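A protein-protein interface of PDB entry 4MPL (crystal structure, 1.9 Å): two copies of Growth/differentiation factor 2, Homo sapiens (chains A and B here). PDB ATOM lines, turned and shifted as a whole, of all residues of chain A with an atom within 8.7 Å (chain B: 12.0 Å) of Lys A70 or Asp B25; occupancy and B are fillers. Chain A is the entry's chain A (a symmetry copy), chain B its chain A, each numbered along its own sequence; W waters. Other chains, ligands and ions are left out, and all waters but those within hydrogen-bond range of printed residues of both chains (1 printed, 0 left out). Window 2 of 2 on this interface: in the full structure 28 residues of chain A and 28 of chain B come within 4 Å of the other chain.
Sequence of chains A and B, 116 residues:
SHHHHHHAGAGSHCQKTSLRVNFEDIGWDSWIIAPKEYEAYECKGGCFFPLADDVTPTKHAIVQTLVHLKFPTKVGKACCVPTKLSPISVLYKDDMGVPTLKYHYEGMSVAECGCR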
ATOM      1  N   VAL A  63      -6.124  -7.796  -9.066  1.00  0.00           N
ATOM      2  CA  VAL A  63      -6.138  -8.300 -10.439  1.00  0.00           C
ATOM      3  C   VAL A  63      -5.277  -7.445 -11.373  1.00  0.00           C
ATOM      4  O   VAL A  63      -4.459  -7.955 -12.144  1.00  0.00           O
ATOM      5  CB  VAL A  63      -7.587  -8.386 -10.971  1.00  0.00           C
ATOM      6  CG1 VAL A  63      -7.597  -8.550 -12.475  1.00  0.00           C
ATOM      7  CG2 VAL A  63      -8.312  -9.551 -10.294  1.00  0.00           C
ATOM      8  N   GLN A  64      -5.448  -6.141 -11.310  1.00  0.00           N
ATOM      9  CA  GLN A  64      -4.694  -5.280 -12.211  1.00  0.00           C
ATOM     10  C   GLN A  64      -3.193  -5.374 -11.930  1.00  0.00           C
ATOM     11  O   GLN A  64      -2.375  -5.315 -12.855  1.00  0.00           O
ATOM     12  CB  GLN A  64      -5.163  -3.828 -12.088  1.00  0.00           C
ATOM     13  CG  GLN A  64      -4.418  -2.911 -13.061  1.00  0.00           C
ATOM     14  CD  GLN A  64      -5.162  -1.655 -13.382  1.00  0.00           C
ATOM     15  OE1 GLN A  64      -6.374  -1.577 -13.199  1.00  0.00           O
ATOM     16  NE2 GLN A  64      -4.443  -0.652 -13.874  1.00  0.00           N
ATOM     17  N   THR A  65      -2.837  -5.552 -10.659  1.00  0.00           N
ATOM     18  CA  THR A  65      -1.415  -5.632 -10.285  1.00  0.00           C
ATOM     19  C   THR A  65      -0.802  -6.871 -10.934  1.00  0.00           C
ATOM     20  O   THR A  65       0.296  -6.823 -11.499  1.00  0.00           O
ATOM     21  CB  THR A  65      -1.248  -5.673  -8.764  1.00  0.00           C
ATOM     22  OG1 THR A  65      -1.775  -4.466  -8.198  1.00  0.00           O
ATOM     23  CG2 THR A  65       0.235  -5.799  -8.376  1.00  0.00           C
ATOM     24  N   LEU A  66      -1.532  -7.981 -10.874  1.00  0.00           N
ATOM     25  CA  LEU A  66      -1.086  -9.219 -11.511  1.00  0.00           C
ATOM     26  C   LEU A  66      -0.976  -9.102 -13.021  1.00  0.00           C
ATOM     27  O   LEU A  66      -0.022  -9.608 -13.617  1.00  0.00           O
ATOM     28  CB  LEU A  66      -2.035 -10.370 -11.136  1.00  0.00           C
ATOM     29  CG  LEU A  66      -2.037 -10.771  -9.661  1.00  0.00           C
ATOM     30  CD1 LEU A  66      -3.257 -11.641  -9.327  1.00  0.00           C
ATOM     31  CD2 LEU A  66      -0.746 -11.502  -9.304  1.00  0.00           C
ATOM     32  N   VAL A  67      -1.952  -8.465 -13.661  1.00  0.00           N
ATOM     33  CA  VAL A  67      -1.898  -8.342 -15.114  1.00  0.00           C
ATOM     34  C   VAL A  67      -0.738  -7.430 -15.503  1.00  0.00           C
ATOM     35  O   VAL A  67      -0.046  -7.680 -16.496  1.00  0.00           O
ATOM     36  CB  VAL A  67      -3.221  -7.796 -15.705  1.00  0.00           C
ATOM     37  CG1 VAL A  67      -3.095  -7.603 -17.210  1.00  0.00           C
ATOM     38  CG2 VAL A  67      -4.365  -8.757 -15.393  1.00  0.00           C
ATOM     39  N   HIS A  68      -0.528  -6.378 -14.722  1.00  0.00           N
ATOM     40  CA  HIS A  68       0.570  -5.458 -15.012  1.00  0.00           C
ATOM     41  C   HIS A  68       1.919  -6.159 -14.891  1.00  0.00           C
ATOM     42  O   HIS A  68       2.822  -5.916 -15.678  1.00  0.00           O
ATOM     43  CB  HIS A  68       0.556  -4.268 -14.076  1.00  0.00           C
ATOM     44  CG  HIS A  68       1.772  -3.412 -14.211  1.00  0.00           C
ATOM     45  ND1 HIS A  68       1.962  -2.564 -15.282  1.00  0.00           N
ATOM     46  CD2 HIS A  68       2.890  -3.320 -13.452  1.00  0.00           C
ATOM     47  CE1 HIS A  68       3.131  -1.957 -15.155  1.00  0.00           C
ATOM     48  NE2 HIS A  68       3.717  -2.404 -14.058  1.00  0.00           N
ATOM     49  N   LEU A  69       2.049  -7.036 -13.906  1.00  0.00           N
ATOM     50  CA  LEU A  69       3.299  -7.777 -13.727  1.00  0.00           C
ATOM     51  C   LEU A  69       3.545  -8.647 -14.954  1.00  0.00           C
ATOM     52  O   LEU A  69       4.649  -8.689 -15.507  1.00  0.00           O
ATOM     53  CB  LEU A  69       3.207  -8.631 -12.464  1.00  0.00           C
ATOM     54  CG  LEU A  69       4.497  -9.306 -12.025  1.00  0.00           C
ATOM     55  CD1 LEU A  69       5.504  -8.257 -11.563  1.00  0.00           C
ATOM     56  CD2 LEU A  69       4.186 -10.273 -10.926  1.00  0.00           C
ATOM     57  N   LYS A  70       2.487  -9.305 -15.410  1.00  0.00           N
ATOM     58  CA  LYS A  70       2.565 -10.192 -16.562  1.00  0.00           C
ATOM     59  C   LYS A  70       2.749  -9.454 -17.893  1.00  0.00           C
ATOM     60  O   LYS A  70       3.552  -9.868 -18.736  1.00  0.00           O
ATOM     61  CB  LYS A  70       1.294 -11.043 -16.607  1.00  0.00           C
ATOM     62  CG  LYS A  70       1.350 -12.207 -17.557  1.00  0.00           C
ATOM     63  CD  LYS A  70       1.995 -13.411 -16.922  1.00  0.00           C
ATOM     64  CE  LYS A  70       1.733 -14.635 -17.769  1.00  0.00           C
ATOM     65  NZ  LYS A  70       2.869 -15.589 -17.696  1.00  0.00           N
ATOM     66  N   PHE A  71       2.003  -8.367 -18.076  1.00  0.00           N
ATOM     67  CA  PHE A  71       1.981  -7.633 -19.342  1.00  0.00           C
ATOM     68  C   PHE A  71       2.158  -6.135 -19.113  1.00  0.00           C
ATOM     69  O   PHE A  71       1.221  -5.358 -19.332  1.00  0.00           O
ATOM     70  CB  PHE A  71       0.662  -7.908 -20.083  1.00  0.00           C
ATOM     71  CG  PHE A  71       0.394  -9.372 -20.318  1.00  0.00           C
ATOM     72  CD1 PHE A  71       1.229 -10.120 -21.137  1.00  0.00           C
ATOM     73  CD2 PHE A  71      -0.691 -10.003 -19.726  1.00  0.00           C
ATOM     74  CE1 PHE A  71       0.994 -11.472 -21.358  1.00  0.00           C
ATOM     75  CE2 PHE A  71      -0.936 -11.353 -19.946  1.00  0.00           C
ATOM     76  CZ  PHE A  71      -0.091 -12.088 -20.759  1.00  0.00           C
ATOM     77  N   PRO A  72       3.371  -5.722 -18.692  1.00  0.00           N
ATOM     78  CA  PRO A  72       3.642  -4.374 -18.163  1.00  0.00           C
ATOM     79  C   PRO A  72       3.446  -3.238 -19.152  1.00  0.00           C
ATOM     80  O   PRO A  72       3.143  -2.122 -18.726  1.00  0.00           O
ATOM     81  CB  PRO A  72       5.112  -4.448 -17.726  1.00  0.00           C
ATOM     82  CG  PRO A  72       5.686  -5.594 -18.462  1.00  0.00           C
ATOM     83  CD  PRO A  72       4.569  -6.578 -18.640  1.00  0.00           C
ATOM     84  N   THR A  73       3.617  -3.515 -20.440  1.00  0.00           N
ATOM     85  CA  THR A  73       3.515  -2.471 -21.459  1.00  0.00           C
ATOM     86  C   THR A  73       2.070  -2.165 -21.849  1.00  0.00           C
ATOM     87  O   THR A  73       1.811  -1.186 -22.554  1.00  0.00           O
ATOM     88  CB  THR A  73       4.289  -2.850 -22.738  1.00  0.00           C
ATOM     89  OG1 THR A  73       3.760  -4.074 -23.276  1.00  0.00           O
ATOM     90  CG2 THR A  73       5.767  -3.021 -22.434  1.00  0.00           C
ATOM     91  N   LYS A  74       1.132  -2.991 -21.394  1.00  0.00           N
ATOM     92  CA  LYS A  74      -0.235  -2.905 -21.899  1.00  0.00           C
ATOM     93  C   LYS A  74      -1.364  -2.782 -20.853  1.00  0.00           C
ATOM     94  O   LYS A  74      -2.532  -2.587 -21.209  1.00  0.00           O
ATOM     95  CB  LYS A  74      -0.473  -4.030 -22.905  1.00  0.00           C
ATOM     96  CG  LYS A  74       0.260  -3.760 -24.213  1.00  0.00           C
ATOM     97  CD  LYS A  74       0.533  -5.012 -25.023  1.00  0.00           C
ATOM     98  CE  LYS A  74       1.230  -4.646 -26.331  1.00  0.00           C
ATOM     99  NZ  LYS A  74       1.975  -5.793 -26.929  1.00  0.00           N
ATOM    100  N   VAL A  75      -1.018  -2.895 -19.574  1.00  0.00           N
ATOM    101  CA  VAL A  75      -1.877  -2.371 -18.519  1.00  0.00           C
ATOM    102  C   VAL A  75      -0.981  -1.744 -17.466  1.00  0.00           C
ATOM    103  O   VAL A  75       0.094  -2.270 -17.153  1.00  0.00           O
ATOM    104  CB  VAL A  75      -2.822  -3.437 -17.885  1.00  0.00           C
ATOM    105  CG1 VAL A  75      -2.110  -4.274 -16.902  1.00  0.00           C
ATOM    106  CG2 VAL A  75      -3.948  -2.764 -17.151  1.00  0.00           C
ATOM    107  N   LEU B  19     -10.613  -4.176 -20.440  1.00  0.00           N
ATOM    108  CA  LEU B  19      -9.480  -5.003 -20.023  1.00  0.00           C
ATOM    109  C   LEU B  19      -9.998  -6.399 -19.757  1.00  0.00           C
ATOM    110  O   LEU B  19     -10.639  -6.639 -18.730  1.00  0.00           O
ATOM    111  CB  LEU B  19      -8.822  -4.464 -18.743  1.00  0.00           C
ATOM    112  CG  LEU B  19      -7.658  -5.306 -18.199  1.00  0.00           C
ATOM    113  CD1 LEU B  19      -6.521  -5.300 -19.197  1.00  0.00           C
ATOM    114  CD2 LEU B  19      -7.173  -4.798 -16.836  1.00  0.00           C
ATOM    115  N   ARG B  20      -9.724  -7.319 -20.677  1.00  0.00           N
ATOM    116  CA  ARG B  20     -10.116  -8.717 -20.482  1.00  0.00           C
ATOM    117  C   ARG B  20      -9.015  -9.457 -19.740  1.00  0.00           C
ATOM    118  O   ARG B  20      -7.849  -9.388 -20.133  1.00  0.00           O
ATOM    119  CB  ARG B  20     -10.401  -9.413 -21.820  1.00  0.00           C
ATOM    120  CG  ARG B  20     -11.699  -8.951 -22.516  1.00  0.00           C
ATOM    121  CD  ARG B  20     -12.568 -10.136 -22.983  1.00  0.00           C
ATOM    122  NE  ARG B  20     -13.805 -10.256 -22.205  1.00  0.00           N
ATOM    123  CZ  ARG B  20     -14.211 -11.373 -21.606  1.00  0.00           C
ATOM    124  NH1 ARG B  20     -15.350 -11.388 -20.909  1.00  0.00           N
ATOM    125  NH2 ARG B  20     -13.486 -12.484 -21.711  1.00  0.00           N
ATOM    126  N   VAL B  21      -9.391 -10.162 -18.678  1.00  0.00           N
ATOM    127  CA  VAL B  21      -8.426 -10.865 -17.832  1.00  0.00           C
ATOM    128  C   VAL B  21      -8.611 -12.383 -17.879  1.00  0.00           C
ATOM    129  O   VAL B  21      -9.713 -12.882 -17.634  1.00  0.00           O
ATOM    130  CB  VAL B  21      -8.543 -10.403 -16.377  1.00  0.00           C
ATOM    131  CG1 VAL B  21      -7.630 -11.231 -15.476  1.00  0.00           C
ATOM    132  CG2 VAL B  21      -8.187  -8.910 -16.270  1.00  0.00           C
ATOM    133  N   ASN B  22      -7.527 -13.099 -18.184  1.00  0.00           N
ATOM    134  CA  ASN B  22      -7.496 -14.566 -18.176  1.00  0.00           C
ATOM    135  C   ASN B  22      -7.000 -15.084 -16.828  1.00  0.00           C
ATOM    136  O   ASN B  22      -5.871 -14.785 -16.407  1.00  0.00           O
ATOM    137  CB  ASN B  22      -6.573 -15.047 -19.291  1.00  0.00           C
ATOM    138  CG  ASN B  22      -6.509 -16.549 -19.388  1.00  0.00           C
ATOM    139  OD1 ASN B  22      -5.926 -17.216 -18.528  1.00  0.00           O
ATOM    140  ND2 ASN B  22      -7.102 -17.096 -20.443  1.00  0.00           N
ATOM    141  N   PHE B  23      -7.832 -15.860 -16.140  1.00  0.00           N
ATOM    142  CA  PHE B  23      -7.480 -16.285 -14.794  1.00  0.00           C
ATOM    143  C   PHE B  23      -6.226 -17.160 -14.730  1.00  0.00           C
ATOM    144  O   PHE B  23      -5.476 -17.091 -13.762  1.00  0.00           O
ATOM    145  CB  PHE B  23      -8.656 -16.980 -14.135  1.00  0.00           C
ATOM    146  CG  PHE B  23      -9.757 -16.039 -13.732  1.00  0.00           C
ATOM    147  CD1 PHE B  23      -9.545 -15.082 -12.747  1.00  0.00           C
ATOM    148  CD2 PHE B  23     -11.002 -16.111 -14.337  1.00  0.00           C
ATOM    149  CE1 PHE B  23     -10.568 -14.206 -12.366  1.00  0.00           C
ATOM    150  CE2 PHE B  23     -12.023 -15.244 -13.959  1.00  0.00           C
ATOM    151  CZ  PHE B  23     -11.806 -14.299 -12.969  1.00  0.00           C
ATOM    152  N   GLU B  24      -5.994 -17.968 -15.756  1.00  0.00           N
ATOM    153  CA  GLU B  24      -4.777 -18.779 -15.785  1.00  0.00           C
ATOM    154  C   GLU B  24      -3.553 -17.883 -15.824  1.00  0.00           C
ATOM    155  O   GLU B  24      -2.597 -18.098 -15.068  1.00  0.00           O
ATOM    156  CB  GLU B  24      -4.762 -19.726 -16.979  1.00  0.00           C
ATOM    157  CG  GLU B  24      -3.454 -20.504 -17.106  1.00  0.00           C
ATOM    158  CD  GLU B  24      -3.503 -21.597 -18.155  1.00  0.00           C
ATOM    159  OE1 GLU B  24      -4.409 -21.562 -19.015  1.00  0.00           O
ATOM    160  OE2 GLU B  24      -2.631 -22.492 -18.117  1.00  0.00           O
ATOM    161  N   ASP B  25      -3.597 -16.865 -16.681  1.00  0.00           N
ATOM    162  CA  ASP B  25      -2.487 -15.936 -16.814  1.00  0.00           C
ATOM    163  C   ASP B  25      -2.093 -15.260 -15.503  1.00  0.00           C
ATOM    164  O   ASP B  25      -0.913 -14.978 -15.287  1.00  0.00           O
ATOM    165  CB  ASP B  25      -2.791 -14.871 -17.863  1.00  0.00           C
ATOM    166  CG  ASP B  25      -2.796 -15.428 -19.260  1.00  0.00           C
ATOM    167  OD1 ASP B  25      -2.432 -16.613 -19.425  1.00  0.00           O
ATOM    168  OD2 ASP B  25      -3.164 -14.679 -20.193  1.00  0.00           O
ATOM    169  N   ILE B  26      -3.065 -14.984 -14.633  1.00  0.00           N
ATOM    170  CA  ILE B  26      -2.754 -14.339 -13.353  1.00  0.00           C
ATOM    171  C   ILE B  26      -2.620 -15.321 -12.178  1.00  0.00           C
ATOM    172  O   ILE B  26      -2.607 -14.905 -11.019  1.00  0.00           O
ATOM    173  CB  ILE B  26      -3.744 -13.197 -12.995  1.00  0.00           C
ATOM    174  CG1 ILE B  26      -5.143 -13.743 -12.691  1.00  0.00           C
ATOM    175  CG2 ILE B  26      -3.770 -12.173 -14.109  1.00  0.00           C
ATOM    176  CD1 ILE B  26      -6.060 -12.717 -11.972  1.00  0.00           C
ATOM    177  N   GLY B  27      -2.515 -16.615 -12.477  1.00  0.00           N
ATOM    178  CA  GLY B  27      -2.213 -17.611 -11.452  1.00  0.00           C
ATOM    179  C   GLY B  27      -3.375 -18.080 -10.589  1.00  0.00           C
ATOM    180  O   GLY B  27      -3.163 -18.703  -9.544  1.00  0.00           O
ATOM    181  N   TRP B  28      -4.605 -17.801 -11.022  1.00  0.00           N
ATOM    182  CA  TRP B  28      -5.776 -18.118 -10.213  1.00  0.00           C
ATOM    183  C   TRP B  28      -6.555 -19.376 -10.635  1.00  0.00           C
ATOM    184  O   TRP B  28      -7.583 -19.687 -10.032  1.00  0.00           O
ATOM    185  CB  TRP B  28      -6.738 -16.923 -10.206  1.00  0.00           C
ATOM    186  CG  TRP B  28      -6.299 -15.804  -9.330  1.00  0.00           C
ATOM    187  CD1 TRP B  28      -5.090 -15.673  -8.701  1.00  0.00           C
ATOM    188  CD2 TRP B  28      -7.071 -14.659  -8.960  1.00  0.00           C
ATOM    189  NE1 TRP B  28      -5.062 -14.504  -7.973  1.00  0.00           N
ATOM    190  CE2 TRP B  28      -6.269 -13.865  -8.118  1.00  0.00           C
ATOM    191  CE3 TRP B  28      -8.364 -14.223  -9.271  1.00  0.00           C
ATOM    192  CZ2 TRP B  28      -6.725 -12.663  -7.568  1.00  0.00           C
ATOM    193  CZ3 TRP B  28      -8.809 -13.028  -8.732  1.00  0.00           C
ATOM    194  CH2 TRP B  28      -7.997 -12.262  -7.895  1.00  0.00           C
ATOM    195  N   ASP B  29      -6.086 -20.102 -11.645  1.00  0.00           N
ATOM    196  CA  ASP B  29      -6.909 -21.185 -12.186  1.00  0.00           C
ATOM    197  C   ASP B  29      -7.016 -22.450 -11.311  1.00  0.00           C
ATOM    198  O   ASP B  29      -7.810 -23.340 -11.619  1.00  0.00           O
ATOM    199  CB  ASP B  29      -6.531 -21.520 -13.642  1.00  0.00           C
ATOM    200  CG  ASP B  29      -5.203 -22.255 -13.760  1.00  0.00           C
ATOM    201  OD1 ASP B  29      -4.666 -22.741 -12.739  1.00  0.00           O
ATOM    202  OD2 ASP B  29      -4.686 -22.348 -14.893  1.00  0.00           O
ATOM    203  N   SER B  30      -6.228 -22.534 -10.237  1.00  0.00           N
ATOM    204  CA  SER B  30      -6.319 -23.686  -9.330  1.00  0.00           C
ATOM    205  C   SER B  30      -7.485 -23.476  -8.391  1.00  0.00           C
ATOM    206  O   SER B  30      -7.908 -24.390  -7.673  1.00  0.00           O
ATOM    207  CB  SER B  30      -5.039 -23.864  -8.509  1.00  0.00           C
ATOM    208  OG  SER B  30      -4.840 -22.776  -7.615  1.00  0.00           O
ATOM    209  N   TRP B  31      -8.008 -22.257  -8.415  1.00  0.00           N
ATOM    210  CA  TRP B  31      -9.015 -21.822  -7.466  1.00  0.00           C
ATOM    211  C   TRP B  31     -10.274 -21.348  -8.202  1.00  0.00           C
ATOM    212  O   TRP B  31     -11.384 -21.568  -7.728  1.00  0.00           O
ATOM    213  CB  TRP B  31      -8.396 -20.733  -6.592  1.00  0.00           C
ATOM    214  CG  TRP B  31      -9.329 -19.829  -5.884  1.00  0.00           C
ATOM    215  CD1 TRP B  31     -10.387 -20.177  -5.089  1.00  0.00           C
ATOM    216  CD2 TRP B  31      -9.255 -18.403  -5.859  1.00  0.00           C
ATOM    217  NE1 TRP B  31     -10.993 -19.042  -4.592  1.00  0.00           N
ATOM    218  CE2 TRP B  31     -10.312 -17.941  -5.048  1.00  0.00           C
ATOM    219  CE3 TRP B  31      -8.398 -17.470  -6.452  1.00  0.00           C
ATOM    220  CZ2 TRP B  31     -10.537 -16.583  -4.819  1.00  0.00           C
ATOM    221  CZ3 TRP B  31      -8.620 -16.123  -6.220  1.00  0.00           C
ATOM    222  CH2 TRP B  31      -9.680 -15.692  -5.412  1.00  0.00           C
ATOM    223  N   ILE B  32     -10.100 -20.732  -9.372  1.00  0.00           N
ATOM    224  CA  ILE B  32     -11.245 -20.317 -10.193  1.00  0.00           C
ATOM    225  C   ILE B  32     -11.389 -21.201 -11.438  1.00  0.00           C
ATOM    226  O   ILE B  32     -10.574 -21.136 -12.357  1.00  0.00           O
ATOM    227  CB  ILE B  32     -11.179 -18.803 -10.543  1.00  0.00           C
ATOM    228  CG1 ILE B  32     -11.197 -17.978  -9.252  1.00  0.00           C
ATOM    229  CG2 ILE B  32     -12.350 -18.392 -11.436  1.00  0.00           C
ATOM    230  CD1 ILE B  32     -11.273 -16.488  -9.453  1.00  0.00           C
ATOM    231  N   ILE B  33     -12.428 -22.038 -11.447  1.00  0.00           N
ATOM    232  CA  ILE B  33     -12.657 -23.020 -12.519  1.00  0.00           C
ATOM    233  C   ILE B  33     -13.289 -22.362 -13.728  1.00  0.00           C
ATOM    234  O   ILE B  33     -13.018 -22.725 -14.877  1.00  0.00           O
ATOM    235  CB  ILE B  33     -13.640 -24.133 -12.067  1.00  0.00           C
ATOM    236  CG1 ILE B  33     -13.264 -24.680 -10.688  1.00  0.00           C
ATOM    237  CG2 ILE B  33     -13.698 -25.263 -13.095  1.00  0.00           C
ATOM    238  CD1 ILE B  33     -14.336 -25.555 -10.064  1.00  0.00           C
ATOM    239  N   ALA B  34     -14.162 -21.402 -13.449  1.00  0.00           N
ATOM    240  CA  ALA B  34     -14.932 -20.742 -14.488  1.00  0.00           C
ATOM    241  C   ALA B  34     -15.398 -19.394 -13.975  1.00  0.00           C
ATOM    242  O   ALA B  34     -15.664 -19.238 -12.775  1.00  0.00           O
ATOM    243  CB  ALA B  34     -16.132 -21.599 -14.883  1.00  0.00           C
ATOM    244  N   PRO B  35     -15.502 -18.406 -14.877  1.00  0.00           N
ATOM    245  CA  PRO B  35     -15.151 -18.468 -16.301  1.00  0.00           C
ATOM    246  C   PRO B  35     -13.640 -18.491 -16.498  1.00  0.00           C
ATOM    247  O   PRO B  35     -12.907 -18.342 -15.514  1.00  0.00           O
ATOM    248  CB  PRO B  35     -15.703 -17.154 -16.847  1.00  0.00           C
ATOM    249  CG  PRO B  35     -15.673 -16.212 -15.656  1.00  0.00           C
ATOM    250  CD  PRO B  35     -15.946 -17.059 -14.457  1.00  0.00           C
ATOM    251  N   LYS B  36     -13.194 -18.652 -17.742  1.00  0.00           N
ATOM    252  CA  LYS B  36     -11.769 -18.696 -18.051  1.00  0.00           C
ATOM    253  C   LYS B  36     -11.194 -17.293 -18.113  1.00  0.00           C
ATOM    254  O   LYS B  36     -10.011 -17.082 -17.836  1.00  0.00           O
ATOM    255  CB  LYS B  36     -11.538 -19.358 -19.405  1.00  0.00           C
ATOM    256  CG  LYS B  36     -11.984 -20.816 -19.503  1.00  0.00           C
ATOM    257  CD  LYS B  36     -11.219 -21.726 -18.551  1.00  0.00           C
ATOM    258  CE  LYS B  36     -11.292 -23.187 -19.008  1.00  0.00           C
ATOM    259  NZ  LYS B  36     -10.542 -24.114 -18.103  1.00  0.00           N
ATOM    260  N   GLU B  37     -12.045 -16.350 -18.506  1.00  0.00           N
ATOM    261  CA  GLU B  37     -11.662 -14.960 -18.734  1.00  0.00           C
ATOM    262  C   GLU B  37     -12.845 -14.100 -18.318  1.00  0.00           C
ATOM    263  O   GLU B  37     -13.983 -14.577 -18.309  1.00  0.00           O
ATOM    264  CB  GLU B  37     -11.372 -14.714 -20.215  1.00  0.00           C
ATOM    265  CG  GLU B  37     -10.036 -15.237 -20.702  1.00  0.00           C
ATOM    266  N   TYR B  38     -12.594 -12.844 -17.963  1.00  0.00           N
ATOM    267  CA  TYR B  38     -13.694 -11.917 -17.723  1.00  0.00           C
ATOM    268  C   TYR B  38     -13.307 -10.492 -18.074  1.00  0.00           C
ATOM    269  O   TYR B  38     -12.130 -10.181 -18.226  1.00  0.00           O
ATOM    270  CB  TYR B  38     -14.193 -12.007 -16.281  1.00  0.00           C
ATOM    271  CG  TYR B  38     -13.438 -11.154 -15.278  1.00  0.00           C
ATOM    272  CD1 TYR B  38     -12.162 -11.511 -14.846  1.00  0.00           C
ATOM    273  CD2 TYR B  38     -14.023 -10.022 -14.727  1.00  0.00           C
ATOM    274  CE1 TYR B  38     -11.488 -10.747 -13.901  1.00  0.00           C
ATOM    275  CE2 TYR B  38     -13.370  -9.265 -13.791  1.00  0.00           C
ATOM    276  CZ  TYR B  38     -12.097  -9.632 -13.378  1.00  0.00           C
ATOM    277  OH  TYR B  38     -11.438  -8.863 -12.440  1.00  0.00           O
ATOM    278  N   ALA B  40     -12.658  -7.199 -16.835  1.00  0.00           N
ATOM    279  CA  ALA B  40     -12.392  -6.450 -15.600  1.00  0.00           C
ATOM    280  C   ALA B  40     -12.516  -4.943 -15.806  1.00  0.00           C
ATOM    281  O   ALA B  40     -12.783  -4.201 -14.851  1.00  0.00           O
ATOM    282  CB  ALA B  40     -10.994  -6.781 -15.070  1.00  0.00           C
HETATM  283  O   HOH W   1       1.050 -16.897 -15.599  1.00  0.00           O
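The backbone carbonyl oxygen (O) of Leu B19 sits at hydrogen-bond distance from the backbone NH (N) of Ala B40 (2.8 Å). The backbone carbonyl oxygen (O) of Tyr B38 is in hydrogen-bond range of the backbone NH (N) of Val B21. The backbone NH of Asp B25 sits at hydrogen-bond distance from the side-chain amide oxygen of Asn B22. O of Phe B23 sits at hydrogen-bond distance from N of Trp B28 (3.0 Å). A ring nitrogen (ND1) of His A68 sits at hydrogen-bond distance from the backbone carbonyl oxygen (O) of Val A75 (2.7 Å).
Val A63 touches Val B21. CG2 of Val A63 touches CH2 of Trp B28, at 3.6 Å. Val A63 touches Tyr B38. Leu A66 touches Ile B26 (CD1 to O, 3.7 Å). Trp B28 touches Leu A66. CG2 of Val B21 touches CG2 of Val A67 (3.9 Å). CG2 of Ile B26 touches CG2 of Val A67 (3.7 Å). O of Asp B25 touches CE of Lys A70, 3.6 Å away. Leu B19 touches Val A75 (CD2 to CG2, 3.8 Å).
Of chain B, only Asp B25 comes within 4 Å of Lys A70. Printed residues of chain A within 4 Å of Asp B25: Lys A70. Of chain B, only Ile B26 and Trp B28 come within 4 Å of Leu A66. Printed residues of chain B within 4 Å of Val A67: Val B21 (3.9 Å) and Ile B26 (3.7 Å). No residue of chain B comes within 4 Å of His A68. Of the printed residues of chain A, Trp B28 touches Val A63 (3.6 Å) and Leu A66 (3.6 Å). Of the printed residues of chain A, Tyr B38 touches Val A63. The nearest printed residue of chain A that does not touch Val B21 is Gln A64 (6.3 Å).
Printed residues of chain A that touch a printed residue of chain B: Val A63, Leu A66, Val A67, Lys A70 and Val A75. Along chain A the printed residues that touch a printed residue of chain B span positions 63 to 75. Of the 21 printed residues of chain B, 6 touch a printed residue of chain A. Among the printed residues, 9 pairs touch across the chains.
No position is printed for both chains. Of the 9 pairs that touch across the chains among the printed residues, none has its exchanged pair printed and touching as well.
Water W1 lies within hydrogen-bond range of O of Asp B25 and NZ of Lys A70.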
